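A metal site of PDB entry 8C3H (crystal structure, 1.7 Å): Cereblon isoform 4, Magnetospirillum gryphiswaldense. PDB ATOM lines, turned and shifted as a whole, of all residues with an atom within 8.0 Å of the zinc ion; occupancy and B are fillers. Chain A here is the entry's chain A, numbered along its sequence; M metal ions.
N of Gln 29 sits close to SG of Cys 27 (3.6 Å). SG of Cys 27 sits close to NE2 of Gln 92 (3.2 Å). The side-chain sulfur (SG) of Cys 24 sits close to the backbone NH (N) of Gln 26 (3.5 Å). N of Cys 24 lies within hydrogen-bond range of O of Gln 29, at 2.8 Å. The side-chain sulfur of Cys 93 sits close to the backbone NH of Ser 95 (3.5 Å). The backbone NH of Cys 90 lies within hydrogen-bond range of the backbone carbonyl oxygen of Ser 95 (2.8 Å). The backbone NH (N) of Gln 92 sits close to the side-chain sulfur (SG) of Cys 90 (3.5 Å).
The nearest printed residue that does not touch the zinc ion is Gln 26 (4.5 Å).
The zinc ion is bound by SG of Cys 27 (2.3 Å), SG of Cys 24 (2.3 Å), SG of Cys 93 (2.3 Å) and SG of Cys 90 (2.4 Å).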
ATOM      1  N   ARG A  23       0.129  28.365  -7.088  1.00  0.00           N
ATOM      2  CA  ARG A  23      -0.334  28.189  -8.476  1.00  0.00           C
ATOM      3  C   ARG A  23      -0.023  26.752  -8.901  1.00  0.00           C
ATOM      4  O   ARG A  23       0.846  26.134  -8.327  1.00  0.00           O
ATOM      5  CB  ARG A  23       0.372  29.195  -9.381  1.00  0.00           C
ATOM      6  CG  ARG A  23      -0.015  30.647  -9.143  1.00  0.00           C
ATOM      7  CD  ARG A  23       0.674  31.601 -10.090  1.00  0.00           C
ATOM      8  NE  ARG A  23       0.247  32.979  -9.858  1.00  0.00           N
ATOM      9  CZ  ARG A  23      -0.939  33.456 -10.210  1.00  0.00           C
ATOM     10  NH1 ARG A  23      -1.791  32.734 -10.931  1.00  0.00           N
ATOM     11  NH2 ARG A  23      -1.281  34.652  -9.825  1.00  0.00           N
ATOM     12  N   CYS A  24      -0.759  26.254  -9.888  1.00  0.00           N
ATOM     13  CA  CYS A  24      -0.457  24.960 -10.543  1.00  0.00           C
ATOM     14  C   CYS A  24       0.960  25.090 -11.109  1.00  0.00           C
ATOM     15  O   CYS A  24       1.212  26.002 -11.890  1.00  0.00           O
ATOM     16  CB  CYS A  24      -1.473  24.631 -11.620  1.00  0.00           C
ATOM     17  SG  CYS A  24      -1.027  23.153 -12.587  1.00  0.00           S
ATOM     18  N   ARG A  25       1.862  24.175 -10.775  1.00  0.00           N
ATOM     19  CA  ARG A  25       3.262  24.179 -11.271  1.00  0.00           C
ATOM     20  C   ARG A  25       3.331  24.000 -12.807  1.00  0.00           C
ATOM     21  O   ARG A  25       4.361  24.359 -13.390  1.00  0.00           O
ATOM     22  CB  ARG A  25       3.969  23.039 -10.528  1.00  0.00           C
ATOM     23  CG  ARG A  25       5.346  22.729 -11.005  1.00  0.00           C
ATOM     24  CD  ARG A  25       5.710  21.435 -10.333  1.00  0.00           C
ATOM     25  NE  ARG A  25       7.020  21.228 -10.818  1.00  0.00           N
ATOM     26  CZ  ARG A  25       7.820  20.325 -10.346  1.00  0.00           C
ATOM     27  NH1 ARG A  25       7.488  19.552  -9.299  1.00  0.00           N
ATOM     28  NH2 ARG A  25       8.945  20.232 -10.975  1.00  0.00           N
ATOM     29  N   GLN A  26       2.317  23.411 -13.412  1.00  0.00           N
ATOM     30  CA  GLN A  26       2.337  23.034 -14.854  1.00  0.00           C
ATOM     31  C   GLN A  26       1.871  24.217 -15.698  1.00  0.00           C
ATOM     32  O   GLN A  26       2.415  24.388 -16.823  1.00  0.00           O
ATOM     33  CB  GLN A  26       1.545  21.763 -15.110  1.00  0.00           C
ATOM     34  CG  GLN A  26       2.124  20.537 -14.436  1.00  0.00           C
ATOM     35  CD  GLN A  26       3.558  20.304 -14.824  1.00  0.00           C
ATOM     36  OE1 GLN A  26       3.962  20.580 -15.956  1.00  0.00           O
ATOM     37  NE2 GLN A  26       4.338  19.861 -13.854  1.00  0.00           N
ATOM     38  N   CYS A  27       0.992  25.071 -15.209  1.00  0.00           N
ATOM     39  CA  CYS A  27       0.373  26.081 -16.092  1.00  0.00           C
ATOM     40  C   CYS A  27       0.156  27.442 -15.401  1.00  0.00           C
ATOM     41  O   CYS A  27      -0.175  28.397 -16.093  1.00  0.00           O
ATOM     42  CB  CYS A  27      -0.946  25.538 -16.606  1.00  0.00           C
ATOM     43  SG  CYS A  27      -2.278  25.545 -15.355  1.00  0.00           S
ATOM     44  N   GLY A  28       0.315  27.560 -14.087  1.00  0.00           N
ATOM     45  CA  GLY A  28       0.201  28.856 -13.385  1.00  0.00           C
ATOM     46  C   GLY A  28      -1.200  29.211 -12.935  1.00  0.00           C
ATOM     47  O   GLY A  28      -1.378  30.285 -12.320  1.00  0.00           O
ATOM     48  N   GLN A  29      -2.183  28.337 -13.124  1.00  0.00           N
ATOM     49  CA  GLN A  29      -3.560  28.548 -12.609  1.00  0.00           C
ATOM     50  C   GLN A  29      -3.488  28.873 -11.100  1.00  0.00           C
ATOM     51  O   GLN A  29      -2.833  28.125 -10.367  1.00  0.00           O
ATOM     52  CB  GLN A  29      -4.438  27.326 -12.853  1.00  0.00           C
ATOM     53  CG  GLN A  29      -5.846  27.395 -12.225  1.00  0.00           C
ATOM     54  CD  GLN A  29      -6.922  27.839 -13.185  1.00  0.00           C
ATOM     55  OE1 GLN A  29      -6.793  28.849 -13.878  1.00  0.00           O
ATOM     56  NE2 GLN A  29      -8.029  27.106 -13.234  1.00  0.00           N
ATOM     57  N   THR A  30      -4.185  29.901 -10.660  1.00  0.00           N
ATOM     58  CA  THR A  30      -4.260  30.238  -9.224  1.00  0.00           C
ATOM     59  C   THR A  30      -5.014  29.157  -8.462  1.00  0.00           C
ATOM     60  O   THR A  30      -6.118  28.852  -8.910  1.00  0.00           O
ATOM     61  CB  THR A  30      -4.985  31.577  -8.996  1.00  0.00           C
ATOM     62  OG1 THR A  30      -4.542  32.516  -9.991  1.00  0.00           O
ATOM     63  CG2 THR A  30      -4.674  32.063  -7.611  1.00  0.00           C
ATOM     64  N   ILE A  31      -4.478  28.602  -7.373  1.00  0.00           N
ATOM     65  CA  ILE A  31      -5.147  27.445  -6.672  1.00  0.00           C
ATOM     66  C   ILE A  31      -5.415  27.792  -5.219  1.00  0.00           C
ATOM     67  O   ILE A  31      -6.558  27.571  -4.753  1.00  0.00           O
ATOM     68  CB  ILE A  31      -4.286  26.179  -6.741  1.00  0.00           C
ATOM     69  CG1 ILE A  31      -3.951  25.779  -8.183  1.00  0.00           C
ATOM     70  CG2 ILE A  31      -4.954  25.036  -5.993  1.00  0.00           C
ATOM     71  CD1 ILE A  31      -5.176  25.390  -8.990  1.00  0.00           C
ATOM     72  N   GLY A  66      -9.858  27.248  -8.837  1.00  0.00           N
ATOM     73  CA  GLY A  66      -9.231  26.928 -10.123  1.00  0.00           C
ATOM     74  C   GLY A  66      -9.104  25.434 -10.331  1.00  0.00           C
ATOM     75  O   GLY A  66      -8.337  25.062 -11.213  1.00  0.00           O
ATOM     76  N   LEU A  89      -8.483  18.060 -10.093  1.00  0.00           N
ATOM     77  CA  LEU A  89      -7.547  18.404 -11.187  1.00  0.00           C
ATOM     78  C   LEU A  89      -7.433  19.933 -11.259  1.00  0.00           C
ATOM     79  O   LEU A  89      -8.328  20.671 -10.818  1.00  0.00           O
ATOM     80  CB  LEU A  89      -8.044  17.863 -12.507  1.00  0.00           C
ATOM     81  CG  LEU A  89      -8.414  16.393 -12.587  1.00  0.00           C
ATOM     82  CD1 LEU A  89      -8.854  16.103 -14.013  1.00  0.00           C
ATOM     83  CD2 LEU A  89      -7.235  15.522 -12.199  1.00  0.00           C
ATOM     84  N   CYS A  90      -6.304  20.397 -11.774  1.00  0.00           N
ATOM     85  CA  CYS A  90      -6.181  21.796 -12.198  1.00  0.00           C
ATOM     86  C   CYS A  90      -7.306  22.007 -13.210  1.00  0.00           C
ATOM     87  O   CYS A  90      -7.383  21.261 -14.224  1.00  0.00           O
ATOM     88  CB  CYS A  90      -4.828  22.014 -12.857  1.00  0.00           C
ATOM     89  SG  CYS A  90      -4.681  23.720 -13.396  1.00  0.00           S
ATOM     90  N   GLY A  91      -8.117  23.057 -13.017  1.00  0.00           N
ATOM     91  CA  GLY A  91      -9.249  23.336 -13.911  1.00  0.00           C
ATOM     92  C   GLY A  91      -8.761  23.823 -15.253  1.00  0.00           C
ATOM     93  O   GLY A  91      -9.529  23.800 -16.219  1.00  0.00           O
ATOM     94  N   GLN A  92      -7.515  24.287 -15.331  1.00  0.00           N
ATOM     95  CA  GLN A  92      -6.942  24.806 -16.594  1.00  0.00           C
ATOM     96  C   GLN A  92      -6.276  23.645 -17.396  1.00  0.00           C
ATOM     97  O   GLN A  92      -6.634  23.436 -18.557  1.00  0.00           O
ATOM     98  CB  GLN A  92      -5.998  25.973 -16.232  1.00  0.00           C
ATOM     99  CG  GLN A  92      -5.340  26.618 -17.428  1.00  0.00           C
ATOM    100  CD  GLN A  92      -4.929  28.039 -17.106  1.00  0.00           C
ATOM    101  OE1 GLN A  92      -5.607  29.012 -17.456  1.00  0.00           O
ATOM    102  NE2 GLN A  92      -3.756  28.147 -16.508  1.00  0.00           N
ATOM    103  N   CYS A  93      -5.263  22.991 -16.833  1.00  0.00           N
ATOM    104  CA  CYS A  93      -4.396  22.039 -17.575  1.00  0.00           C
ATOM    105  C   CYS A  93      -4.762  20.584 -17.288  1.00  0.00           C
ATOM    106  O   CYS A  93      -4.227  19.723 -18.012  1.00  0.00           O
ATOM    107  CB  CYS A  93      -2.916  22.250 -17.376  1.00  0.00           C
ATOM    108  SG  CYS A  93      -2.347  21.681 -15.762  1.00  0.00           S
ATOM    109  N   GLY A  94      -5.641  20.295 -16.331  1.00  0.00           N
ATOM    110  CA  GLY A  94      -6.039  18.896 -16.053  1.00  0.00           C
ATOM    111  C   GLY A  94      -5.009  18.102 -15.230  1.00  0.00           C
ATOM    112  O   GLY A  94      -5.246  16.945 -15.030  1.00  0.00           O
ATOM    113  N   SER A  95      -3.930  18.700 -14.737  1.00  0.00           N
ATOM    114  CA  SER A  95      -2.916  18.060 -13.853  1.00  0.00           C
ATOM    115  C   SER A  95      -3.589  17.607 -12.556  1.00  0.00           C
ATOM    116  O   SER A  95      -4.410  18.350 -12.019  1.00  0.00           O
ATOM    117  CB  SER A  95      -1.784  19.031 -13.558  1.00  0.00           C
ATOM    118  OG  SER A  95      -0.959  18.590 -12.486  1.00  0.00           O
ATOM    119  N   HIS A  96      -3.246  16.422 -12.049  1.00  0.00           N
ATOM    120  CA  HIS A  96      -3.761  15.999 -10.719  1.00  0.00           C
ATOM    121  C   HIS A  96      -3.117  16.836  -9.605  1.00  0.00           C
ATOM    122  O   HIS A  96      -1.910  16.743  -9.405  1.00  0.00           O
ATOM    123  CB  HIS A  96      -3.520  14.496 -10.525  1.00  0.00           C
ATOM    124  CG  HIS A  96      -4.053  14.025  -9.224  1.00  0.00           C
ATOM    125  ND1 HIS A  96      -3.381  13.047  -8.477  1.00  0.00           N
ATOM    126  CD2 HIS A  96      -5.107  14.448  -8.464  1.00  0.00           C
ATOM    127  CE1 HIS A  96      -4.041  12.865  -7.351  1.00  0.00           C
ATOM    128  NE2 HIS A  96      -5.113  13.683  -7.337  1.00  0.00           N
ATOM    129  N   LEU A  97      -3.901  17.599  -8.851  1.00  0.00           N
ATOM    130  CA  LEU A  97      -3.342  18.460  -7.800  1.00  0.00           C
ATOM    131  C   LEU A  97      -3.646  17.943  -6.399  1.00  0.00           C
ATOM    132  O   LEU A  97      -3.004  18.418  -5.450  1.00  0.00           O
ATOM    133  CB  LEU A  97      -3.813  19.912  -7.972  1.00  0.00           C
ATOM    134  CG  LEU A  97      -3.326  20.638  -9.230  1.00  0.00           C
ATOM    135  CD1 LEU A  97      -3.716  22.115  -9.154  1.00  0.00           C
ATOM    136  CD2 LEU A  97      -1.839  20.518  -9.390  1.00  0.00           C
ATOM    137  N   ARG A 117       3.232  19.653  -6.574  1.00  0.00           N
ATOM    138  CA  ARG A 117       2.466  19.988  -7.813  1.00  0.00           C
ATOM    139  C   ARG A 117       2.042  21.447  -7.825  1.00  0.00           C
ATOM    140  O   ARG A 117       1.394  21.847  -8.812  1.00  0.00           O
ATOM    141  CB  ARG A 117       1.308  19.016  -7.973  1.00  0.00           C
ATOM    142  CG  ARG A 117       1.803  17.587  -7.838  1.00  0.00           C
ATOM    143  CD  ARG A 117       1.492  16.659  -8.970  1.00  0.00           C
ATOM    144  NE  ARG A 117       1.809  15.287  -8.561  1.00  0.00           N
ATOM    145  CZ  ARG A 117       1.053  14.236  -8.830  1.00  0.00           C
ATOM    146  NH1 ARG A 117      -0.083  14.379  -9.497  1.00  0.00           N
ATOM    147  NH2 ARG A 117       1.409  13.034  -8.429  1.00  0.00           N
HETATM  148 ZN    ZN M   1      -2.497  23.526 -14.315  1.00  0.00          ZN
